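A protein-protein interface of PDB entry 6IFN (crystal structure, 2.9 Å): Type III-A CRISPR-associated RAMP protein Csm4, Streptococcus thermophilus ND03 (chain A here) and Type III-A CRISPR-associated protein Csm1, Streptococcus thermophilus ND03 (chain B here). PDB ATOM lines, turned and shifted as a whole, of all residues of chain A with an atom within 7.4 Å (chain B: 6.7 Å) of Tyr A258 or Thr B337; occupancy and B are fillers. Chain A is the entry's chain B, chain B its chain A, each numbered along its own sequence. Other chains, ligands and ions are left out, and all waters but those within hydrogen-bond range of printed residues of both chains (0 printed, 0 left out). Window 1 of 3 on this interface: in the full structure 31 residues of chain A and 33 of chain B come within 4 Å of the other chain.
Of the 15 printed residues of chain B, 5 touch a printed residue of chain A. Along chain B the printed residues that touch a printed residue of chain A span positions 337 to 391. Hydrophobic or aromatic side chains of chain A within 4 Å of the printed part of chain B: Leu A219, Leu A225, Leu A236, Leu A257, Tyr A258 and Phe A260. Along chain A the printed residues that touch a printed residue of chain B span positions 219 to 260. Among the printed residues, 9 pairs touch across the chains. Among the printed residues, no Asp or Glu carboxylate lies within 4 Å of a Lys or Arg side-chain nitrogen of the other chain.
OD1 of Asn B391 lies within hydrogen-bond range of N of Tyr A258 (2.5 Å).
The backbone carbonyl oxygen (O) of Ala A218 sits at hydrogen-bond distance from the backbone NH (N) of Phe A260 (3.0 Å). N of Ser A239 lies within hydrogen-bond range of O of Leu A257, at 2.7 Å.
Of the printed residues of chain B, Tyr A258 touches Thr B337, Leu B387, Leu B390 and Asn B391. Thr B337 touches one residue of chain A. Of the printed residues of chain B, Leu A225 touches Leu B387 (3.9 Å). Of the printed residues of chain A, Tyr B382 touches Leu A236. Printed residues of chain B within 4 Å of Leu A219: Asn B391. Of the printed residues of chain B, Phe A260 touches Leu B387 (3.6 Å). Ala A218 touches none of the printed residues of chain B. Arg B338 touches none of the printed residues of chain A. The nearest residue of chain A that does not touch Thr B337 is Lys A238 (5.0 Å).
Among the printed residues, merely in contact across the chains: Leu A219 with Asn B391, Leu A225 with Leu B387, Leu A236 with Tyr B382, Leu A257 with Asn B391, Tyr A258 with Thr B337, Tyr A258 with Leu B387, Tyr A258 with Leu B390 and Phe A260 with Leu B387.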
ATOM      1  N   THR A 217     -40.560  25.681  32.410  1.00  0.00           N
ATOM      2  CA  THR A 217     -39.227  26.110  32.040  1.00  0.00           C
ATOM      3  C   THR A 217     -38.926  27.383  32.831  1.00  0.00           C
ATOM      4  O   THR A 217     -39.525  28.436  32.566  1.00  0.00           O
ATOM      5  CB  THR A 217     -39.074  26.296  30.527  1.00  0.00           C
ATOM      6  OG1 THR A 217     -39.364  25.048  29.896  1.00  0.00           O
ATOM      7  CG2 THR A 217     -37.687  26.754  30.144  1.00  0.00           C
ATOM      8  N   ALA A 218     -37.993  27.258  33.780  1.00  0.00           N
ATOM      9  CA  ALA A 218     -37.979  28.112  34.931  1.00  0.00           C
ATOM     10  C   ALA A 218     -36.550  28.481  35.309  1.00  0.00           C
ATOM     11  O   ALA A 218     -35.625  27.729  35.023  1.00  0.00           O
ATOM     12  CB  ALA A 218     -38.632  27.390  36.076  1.00  0.00           C
ATOM     13  N   LEU A 219     -36.406  29.621  35.988  1.00  0.00           N
ATOM     14  CA  LEU A 219     -35.140  30.080  36.390  1.00  0.00           C
ATOM     15  C   LEU A 219     -35.232  30.344  37.865  1.00  0.00           C
ATOM     16  O   LEU A 219     -36.037  31.144  38.296  1.00  0.00           O
ATOM     17  CB  LEU A 219     -34.779  31.365  35.668  1.00  0.00           C
ATOM     18  CG  LEU A 219     -33.437  31.958  36.088  1.00  0.00           C
ATOM     19  CD1 LEU A 219     -32.267  31.035  35.767  1.00  0.00           C
ATOM     20  CD2 LEU A 219     -33.242  33.300  35.407  1.00  0.00           C
ATOM     21  N   PRO A 220     -34.466  29.631  38.691  1.00  0.00           N
ATOM     22  CA  PRO A 220     -34.402  29.951  40.109  1.00  0.00           C
ATOM     23  C   PRO A 220     -33.895  31.374  40.427  1.00  0.00           C
ATOM     24  O   PRO A 220     -33.070  32.002  39.691  1.00  0.00           O
ATOM     25  CB  PRO A 220     -33.435  28.878  40.642  1.00  0.00           C
ATOM     26  CG  PRO A 220     -33.579  27.725  39.676  1.00  0.00           C
ATOM     27  CD  PRO A 220     -33.742  28.409  38.335  1.00  0.00           C
ATOM     28  N   LEU A 225     -30.060  29.189  43.288  1.00  0.00           N
ATOM     29  CA  LEU A 225     -29.605  28.684  41.987  1.00  0.00           C
ATOM     30  C   LEU A 225     -28.505  27.651  42.194  1.00  0.00           C
ATOM     31  O   LEU A 225     -28.546  26.587  41.604  1.00  0.00           O
ATOM     32  CB  LEU A 225     -29.073  29.820  41.110  1.00  0.00           C
ATOM     33  CG  LEU A 225     -28.662  29.401  39.693  1.00  0.00           C
ATOM     34  CD1 LEU A 225     -29.876  28.959  38.880  1.00  0.00           C
ATOM     35  CD2 LEU A 225     -27.922  30.512  38.973  1.00  0.00           C
ATOM     36  N   LEU A 236     -30.340  23.249  29.834  1.00  0.00           N
ATOM     37  CA  LEU A 236     -30.544  24.725  29.762  1.00  0.00           C
ATOM     38  C   LEU A 236     -31.085  25.120  28.404  1.00  0.00           C
ATOM     39  O   LEU A 236     -30.497  24.798  27.417  1.00  0.00           O
ATOM     40  CB  LEU A 236     -29.226  25.442  29.981  1.00  0.00           C
ATOM     41  CG  LEU A 236     -28.657  25.168  31.358  1.00  0.00           C
ATOM     42  CD1 LEU A 236     -27.314  25.836  31.547  1.00  0.00           C
ATOM     43  CD2 LEU A 236     -29.665  25.598  32.425  1.00  0.00           C
ATOM     44  N   THR A 237     -32.202  25.828  28.364  1.00  0.00           N
ATOM     45  CA  THR A 237     -32.720  26.300  27.100  1.00  0.00           C
ATOM     46  C   THR A 237     -32.557  27.817  27.053  1.00  0.00           C
ATOM     47  O   THR A 237     -32.502  28.459  28.092  1.00  0.00           O
ATOM     48  CB  THR A 237     -34.182  25.899  26.940  1.00  0.00           C
ATOM     49  OG1 THR A 237     -34.934  26.957  27.535  1.00  0.00           O
ATOM     50  CG2 THR A 237     -34.493  24.572  27.589  1.00  0.00           C
ATOM     51  N   LYS A 238     -32.490  28.375  25.850  1.00  0.00           N
ATOM     52  CA  LYS A 238     -32.213  29.762  25.706  1.00  0.00           C
ATOM     53  C   LYS A 238     -33.469  30.472  25.224  1.00  0.00           C
ATOM     54  O   LYS A 238     -33.884  30.224  24.117  1.00  0.00           O
ATOM     55  CB  LYS A 238     -31.093  30.001  24.692  1.00  0.00           C
ATOM     56  CG  LYS A 238     -30.591  31.444  24.656  1.00  0.00           C
ATOM     57  CD  LYS A 238     -29.607  31.778  23.543  1.00  0.00           C
ATOM     58  CE  LYS A 238     -30.290  32.123  22.234  1.00  0.00           C
ATOM     59  NZ  LYS A 238     -29.615  33.284  21.603  1.00  0.00           N
ATOM     60  N   SER A 239     -34.019  31.379  26.035  1.00  0.00           N
ATOM     61  CA  SER A 239     -35.115  32.223  25.593  1.00  0.00           C
ATOM     62  C   SER A 239     -34.569  33.497  24.959  1.00  0.00           C
ATOM     63  O   SER A 239     -33.847  34.270  25.616  1.00  0.00           O
ATOM     64  CB  SER A 239     -36.053  32.542  26.703  1.00  0.00           C
ATOM     65  OG  SER A 239     -36.996  31.495  26.805  1.00  0.00           O
ATOM     66  N   SER A 240     -34.988  33.717  23.712  1.00  0.00           N
ATOM     67  CA  SER A 240     -34.539  34.791  22.920  1.00  0.00           C
ATOM     68  C   SER A 240     -35.656  35.197  21.948  1.00  0.00           C
ATOM     69  O   SER A 240     -36.569  34.456  21.714  1.00  0.00           O
ATOM     70  CB  SER A 240     -33.249  34.401  22.219  1.00  0.00           C
ATOM     71  OG  SER A 240     -33.406  33.229  21.432  1.00  0.00           O
ATOM     72  N   GLN A 255     -33.550  40.497  26.149  1.00  0.00           N
ATOM     73  CA  GLN A 255     -32.340  39.997  26.736  1.00  0.00           C
ATOM     74  C   GLN A 255     -32.389  38.477  26.708  1.00  0.00           C
ATOM     75  O   GLN A 255     -33.367  37.896  27.089  1.00  0.00           O
ATOM     76  CB  GLN A 255     -32.169  40.368  28.217  1.00  0.00           C
ATOM     77  CG  GLN A 255     -32.382  41.834  28.592  1.00  0.00           C
ATOM     78  CD  GLN A 255     -31.371  42.733  27.934  1.00  0.00           C
ATOM     79  OE1 GLN A 255     -30.195  42.377  27.806  1.00  0.00           O
ATOM     80  NE2 GLN A 255     -31.838  43.909  27.520  1.00  0.00           N
ATOM     81  N   ASP A 256     -31.298  37.857  26.274  1.00  0.00           N
ATOM     82  CA  ASP A 256     -31.249  36.432  26.259  1.00  0.00           C
ATOM     83  C   ASP A 256     -31.328  35.954  27.710  1.00  0.00           C
ATOM     84  O   ASP A 256     -30.702  36.552  28.618  1.00  0.00           O
ATOM     85  CB  ASP A 256     -30.001  35.952  25.522  1.00  0.00           C
ATOM     86  CG  ASP A 256     -29.989  36.383  24.061  1.00  0.00           C
ATOM     87  OD1 ASP A 256     -31.118  36.568  23.464  1.00  0.00           O
ATOM     88  OD2 ASP A 256     -28.861  36.548  23.516  1.00  0.00           O
ATOM     89  N   LEU A 257     -32.106  34.886  27.922  1.00  0.00           N
ATOM     90  CA  LEU A 257     -32.251  34.298  29.227  1.00  0.00           C
ATOM     91  C   LEU A 257     -32.116  32.777  29.135  1.00  0.00           C
ATOM     92  O   LEU A 257     -32.845  32.129  28.375  1.00  0.00           O
ATOM     93  CB  LEU A 257     -33.635  34.684  29.729  1.00  0.00           C
ATOM     94  CG  LEU A 257     -33.982  34.146  31.103  1.00  0.00           C
ATOM     95  CD1 LEU A 257     -33.110  34.798  32.149  1.00  0.00           C
ATOM     96  CD2 LEU A 257     -35.443  34.395  31.390  1.00  0.00           C
ATOM     97  N   TYR A 258     -31.222  32.202  29.940  1.00  0.00           N
ATOM     98  CA  TYR A 258     -31.072  30.772  29.979  1.00  0.00           C
ATOM     99  C   TYR A 258     -31.834  30.270  31.201  1.00  0.00           C
ATOM    100  O   TYR A 258     -31.647  30.840  32.314  1.00  0.00           O
ATOM    101  CB  TYR A 258     -29.591  30.401  29.975  1.00  0.00           C
ATOM    102  CG  TYR A 258     -28.872  30.950  28.772  1.00  0.00           C
ATOM    103  CD1 TYR A 258     -28.424  32.257  28.738  1.00  0.00           C
ATOM    104  CD2 TYR A 258     -28.665  30.180  27.647  1.00  0.00           C
ATOM    105  CE1 TYR A 258     -27.771  32.776  27.636  1.00  0.00           C
ATOM    106  CE2 TYR A 258     -28.012  30.676  26.535  1.00  0.00           C
ATOM    107  CZ  TYR A 258     -27.579  31.980  26.527  1.00  0.00           C
ATOM    108  OH  TYR A 258     -26.971  32.486  25.424  1.00  0.00           O
ATOM    109  N   LYS A 259     -32.706  29.270  30.963  1.00  0.00           N
ATOM    110  CA  LYS A 259     -33.530  28.609  31.997  1.00  0.00           C
ATOM    111  C   LYS A 259     -33.339  27.092  31.959  1.00  0.00           C
ATOM    112  O   LYS A 259     -32.826  26.543  31.013  1.00  0.00           O
ATOM    113  CB  LYS A 259     -35.008  28.906  31.781  1.00  0.00           C
ATOM    114  CG  LYS A 259     -35.423  30.320  32.160  1.00  0.00           C
ATOM    115  CD  LYS A 259     -36.102  31.082  31.050  1.00  0.00           C
ATOM    116  CE  LYS A 259     -37.518  30.629  30.787  1.00  0.00           C
ATOM    117  NZ  LYS A 259     -38.202  31.489  29.795  1.00  0.00           N
ATOM    118  N   PHE A 260     -33.805  26.430  33.015  1.00  0.00           N
ATOM    119  CA  PHE A 260     -33.828  24.976  33.131  1.00  0.00           C
ATOM    120  C   PHE A 260     -35.119  24.470  32.483  1.00  0.00           C
ATOM    121  O   PHE A 260     -36.226  24.989  32.744  1.00  0.00           O
ATOM    122  CB  PHE A 260     -33.788  24.532  34.594  1.00  0.00           C
ATOM    123  CG  PHE A 260     -32.579  25.041  35.313  1.00  0.00           C
ATOM    124  CD1 PHE A 260     -32.494  26.358  35.706  1.00  0.00           C
ATOM    125  CD2 PHE A 260     -31.502  24.223  35.548  1.00  0.00           C
ATOM    126  CE1 PHE A 260     -31.355  26.846  36.322  1.00  0.00           C
ATOM    127  CE2 PHE A 260     -30.372  24.707  36.188  1.00  0.00           C
ATOM    128  CZ  PHE A 260     -30.285  26.025  36.552  1.00  0.00           C
ATOM    129  N   SER B 249     -19.976  19.010  22.290  1.00  0.00           N
ATOM    130  CA  SER B 249     -21.410  18.975  21.995  1.00  0.00           C
ATOM    131  C   SER B 249     -21.770  20.228  21.236  1.00  0.00           C
ATOM    132  O   SER B 249     -21.288  21.278  21.563  1.00  0.00           O
ATOM    133  CB  SER B 249     -22.250  18.865  23.215  1.00  0.00           C
ATOM    134  OG  SER B 249     -21.596  18.043  24.162  1.00  0.00           O
ATOM    135  N   GLY B 250     -22.617  20.067  20.233  1.00  0.00           N
ATOM    136  CA  GLY B 250     -23.230  21.204  19.574  1.00  0.00           C
ATOM    137  C   GLY B 250     -22.827  21.347  18.119  1.00  0.00           C
ATOM    138  O   GLY B 250     -23.172  22.366  17.505  1.00  0.00           O
ATOM    139  N   LEU B 331     -14.690  28.306  25.210  1.00  0.00           N
ATOM    140  CA  LEU B 331     -15.913  28.022  24.435  1.00  0.00           C
ATOM    141  C   LEU B 331     -17.058  28.941  24.886  1.00  0.00           C
ATOM    142  O   LEU B 331     -17.948  29.248  24.108  1.00  0.00           O
ATOM    143  CB  LEU B 331     -16.339  26.559  24.635  1.00  0.00           C
ATOM    144  CG  LEU B 331     -15.631  25.496  23.805  1.00  0.00           C
ATOM    145  CD1 LEU B 331     -16.249  24.141  24.080  1.00  0.00           C
ATOM    146  CD2 LEU B 331     -15.702  25.804  22.316  1.00  0.00           C
ATOM    147  N   LEU B 332     -17.082  29.284  26.175  1.00  0.00           N
ATOM    148  CA  LEU B 332     -18.133  30.118  26.681  1.00  0.00           C
ATOM    149  C   LEU B 332     -17.948  31.520  26.115  1.00  0.00           C
ATOM    150  O   LEU B 332     -18.905  32.129  25.618  1.00  0.00           O
ATOM    151  CB  LEU B 332     -18.119  30.127  28.208  1.00  0.00           C
ATOM    152  CG  LEU B 332     -19.333  29.439  28.804  1.00  0.00           C
ATOM    153  CD1 LEU B 332     -19.117  29.122  30.271  1.00  0.00           C
ATOM    154  CD2 LEU B 332     -20.576  30.285  28.593  1.00  0.00           C
ATOM    155  N   PHE B 335     -18.496  31.087  21.881  1.00  0.00           N
ATOM    156  CA  PHE B 335     -19.739  30.540  21.292  1.00  0.00           C
ATOM    157  C   PHE B 335     -20.896  30.472  22.266  1.00  0.00           C
ATOM    158  O   PHE B 335     -21.855  29.898  21.847  1.00  0.00           O
ATOM    159  CB  PHE B 335     -19.474  29.130  20.773  1.00  0.00           C
ATOM    160  CG  PHE B 335     -18.225  29.048  19.945  1.00  0.00           C
ATOM    161  CD1 PHE B 335     -18.245  29.352  18.604  1.00  0.00           C
ATOM    162  CD2 PHE B 335     -17.022  28.736  20.529  1.00  0.00           C
ATOM    163  CE1 PHE B 335     -17.090  29.305  17.858  1.00  0.00           C
ATOM    164  CE2 PHE B 335     -15.868  28.701  19.784  1.00  0.00           C
ATOM    165  CZ  PHE B 335     -15.911  28.970  18.449  1.00  0.00           C
ATOM    166  N   GLN B 336     -20.781  31.032  23.464  1.00  0.00           N
ATOM    167  CA  GLN B 336     -21.849  30.973  24.493  1.00  0.00           C
ATOM    168  C   GLN B 336     -22.143  29.512  24.826  1.00  0.00           C
ATOM    169  O   GLN B 336     -21.245  28.815  25.238  1.00  0.00           O
ATOM    170  CB  GLN B 336     -23.088  31.786  24.112  1.00  0.00           C
ATOM    171  CG  GLN B 336     -22.841  33.280  23.989  1.00  0.00           C
ATOM    172  CD  GLN B 336     -22.320  33.732  22.648  1.00  0.00           C
ATOM    173  OE1 GLN B 336     -22.937  33.525  21.614  1.00  0.00           O
ATOM    174  NE2 GLN B 336     -21.180  34.393  22.656  1.00  0.00           N
ATOM    175  N   THR B 337     -23.391  29.091  24.695  1.00  0.00           N
ATOM    176  CA  THR B 337     -23.795  27.703  25.031  1.00  0.00           C
ATOM    177  C   THR B 337     -23.831  26.790  23.806  1.00  0.00           C
ATOM    178  O   THR B 337     -24.243  25.664  23.954  1.00  0.00           O
ATOM    179  CB  THR B 337     -25.167  27.713  25.690  1.00  0.00           C
ATOM    180  OG1 THR B 337     -25.957  28.622  24.942  1.00  0.00           O
ATOM    181  CG2 THR B 337     -25.117  28.192  27.116  1.00  0.00           C
ATOM    182  N   ARG B 338     -23.442  27.295  22.647  1.00  0.00           N
ATOM    183  CA  ARG B 338     -23.448  26.550  21.368  1.00  0.00           C
ATOM    184  C   ARG B 338     -22.442  25.401  21.319  1.00  0.00           C
ATOM    185  O   ARG B 338     -22.719  24.457  20.636  1.00  0.00           O
ATOM    186  CB  ARG B 338     -23.433  27.516  20.189  1.00  0.00           C
ATOM    187  CG  ARG B 338     -24.583  28.501  20.244  1.00  0.00           C
ATOM    188  CD  ARG B 338     -24.848  29.077  18.884  1.00  0.00           C
ATOM    189  NE  ARG B 338     -23.706  29.822  18.417  1.00  0.00           N
ATOM    190  CZ  ARG B 338     -23.639  31.133  18.360  1.00  0.00           C
ATOM    191  NH1 ARG B 338     -22.555  31.709  17.879  1.00  0.00           N
ATOM    192  NH2 ARG B 338     -24.650  31.865  18.775  1.00  0.00           N
ATOM    193  N   LEU B 339     -21.267  25.547  21.911  1.00  0.00           N
ATOM    194  CA  LEU B 339     -20.287  24.483  21.948  1.00  0.00           C
ATOM    195  C   LEU B 339     -19.913  24.236  23.406  1.00  0.00           C
ATOM    196  O   LEU B 339     -19.716  25.165  24.147  1.00  0.00           O
ATOM    197  CB  LEU B 339     -19.017  24.873  21.181  1.00  0.00           C
ATOM    198  CG  LEU B 339     -19.097  25.059  19.663  1.00  0.00           C
ATOM    199  CD1 LEU B 339     -17.692  25.021  19.103  1.00  0.00           C
ATOM    200  CD2 LEU B 339     -19.940  24.003  18.966  1.00  0.00           C
ATOM    201  N   TYR B 340     -19.790  22.973  23.797  1.00  0.00           N
ATOM    202  CA  TYR B 340     -19.392  22.575  25.142  1.00  0.00           C
ATOM    203  C   TYR B 340     -18.540  21.332  24.959  1.00  0.00           C
ATOM    204  O   TYR B 340     -18.726  20.593  23.990  1.00  0.00           O
ATOM    205  CB  TYR B 340     -20.617  22.301  26.023  1.00  0.00           C
ATOM    206  CG  TYR B 340     -20.354  21.959  27.465  1.00  0.00           C
ATOM    207  CD1 TYR B 340     -20.254  22.943  28.430  1.00  0.00           C
ATOM    208  CD2 TYR B 340     -20.268  20.646  27.895  1.00  0.00           C
ATOM    209  CE1 TYR B 340     -20.022  22.636  29.767  1.00  0.00           C
ATOM    210  CE2 TYR B 340     -20.037  20.319  29.223  1.00  0.00           C
ATOM    211  CZ  TYR B 340     -19.914  21.317  30.171  1.00  0.00           C
ATOM    212  OH  TYR B 340     -19.668  20.995  31.478  1.00  0.00           O
ATOM    213  N   ARG B 381     -24.557  21.299  33.178  1.00  0.00           N
ATOM    214  CA  ARG B 381     -23.461  21.836  32.403  1.00  0.00           C
ATOM    215  C   ARG B 381     -22.684  22.904  33.192  1.00  0.00           C
ATOM    216  O   ARG B 381     -21.451  22.851  33.268  1.00  0.00           O
ATOM    217  CB  ARG B 381     -23.970  22.290  31.028  1.00  0.00           C
ATOM    218  CG  ARG B 381     -23.924  21.202  29.956  1.00  0.00           C
ATOM    219  CD  ARG B 381     -24.834  21.470  28.762  1.00  0.00           C
ATOM    220  NE  ARG B 381     -24.227  21.183  27.461  1.00  0.00           N
ATOM    221  CZ  ARG B 381     -24.546  20.152  26.691  1.00  0.00           C
ATOM    222  NH1 ARG B 381     -25.291  19.178  27.171  1.00  0.00           N
ATOM    223  NH2 ARG B 381     -24.163  20.106  25.427  1.00  0.00           N
ATOM    224  N   TYR B 382     -23.329  23.902  33.762  1.00  0.00           N
ATOM    225  CA  TYR B 382     -22.460  24.943  34.235  1.00  0.00           C
ATOM    226  C   TYR B 382     -22.494  25.057  35.758  1.00  0.00           C
ATOM    227  O   TYR B 382     -23.016  24.187  36.441  1.00  0.00           O
ATOM    228  CB  TYR B 382     -22.854  26.217  33.529  1.00  0.00           C
ATOM    229  CG  TYR B 382     -22.665  26.114  32.047  1.00  0.00           C
ATOM    230  CD1 TYR B 382     -21.402  26.226  31.508  1.00  0.00           C
ATOM    231  CD2 TYR B 382     -23.735  25.944  31.188  1.00  0.00           C
ATOM    232  CE1 TYR B 382     -21.209  26.181  30.143  1.00  0.00           C
ATOM    233  CE2 TYR B 382     -23.559  25.874  29.824  1.00  0.00           C
ATOM    234  CZ  TYR B 382     -22.289  25.993  29.297  1.00  0.00           C
ATOM    235  OH  TYR B 382     -22.058  25.944  27.948  1.00  0.00           O
ATOM    236  N   LEU B 387     -23.878  30.685  34.884  1.00  0.00           N
ATOM    237  CA  LEU B 387     -25.276  30.932  34.524  1.00  0.00           C
ATOM    238  C   LEU B 387     -25.618  32.381  34.877  1.00  0.00           C
ATOM    239  O   LEU B 387     -26.210  33.097  34.046  1.00  0.00           O
ATOM    240  CB  LEU B 387     -26.227  29.955  35.213  1.00  0.00           C
ATOM    241  CG  LEU B 387     -27.671  30.006  34.706  1.00  0.00           C
ATOM    242  CD1 LEU B 387     -27.701  30.048  33.190  1.00  0.00           C
ATOM    243  CD2 LEU B 387     -28.486  28.815  35.213  1.00  0.00           C
ATOM    244  N   LEU B 390     -24.373  34.515  32.081  1.00  0.00           N
ATOM    245  CA  LEU B 390     -25.114  34.355  30.821  1.00  0.00           C
ATOM    246  C   LEU B 390     -26.428  35.154  30.885  1.00  0.00           C
ATOM    247  O   LEU B 390     -26.814  35.792  29.905  1.00  0.00           O
ATOM    248  CB  LEU B 390     -25.418  32.877  30.566  1.00  0.00           C
ATOM    249  CG  LEU B 390     -24.297  32.012  29.995  1.00  0.00           C
ATOM    250  CD1 LEU B 390     -24.632  30.549  30.128  1.00  0.00           C
ATOM    251  CD2 LEU B 390     -24.045  32.315  28.547  1.00  0.00           C
ATOM    252  N   ASN B 391     -27.107  35.137  32.044  1.00  0.00           N
ATOM    253  CA  ASN B 391     -28.373  35.843  32.204  1.00  0.00           C
ATOM    254  C   ASN B 391     -28.198  37.315  32.622  1.00  0.00           C
ATOM    255  O   ASN B 391     -29.175  37.945  33.000  1.00  0.00           O
ATOM    256  CB  ASN B 391     -29.242  35.186  33.265  1.00  0.00           C
ATOM    257  CG  ASN B 391     -29.725  33.833  32.846  1.00  0.00           C
ATOM    258  OD1 ASN B 391     -29.994  33.598  31.683  1.00  0.00           O
ATOM    259  ND2 ASN B 391     -29.888  32.956  33.813  1.00  0.00           N
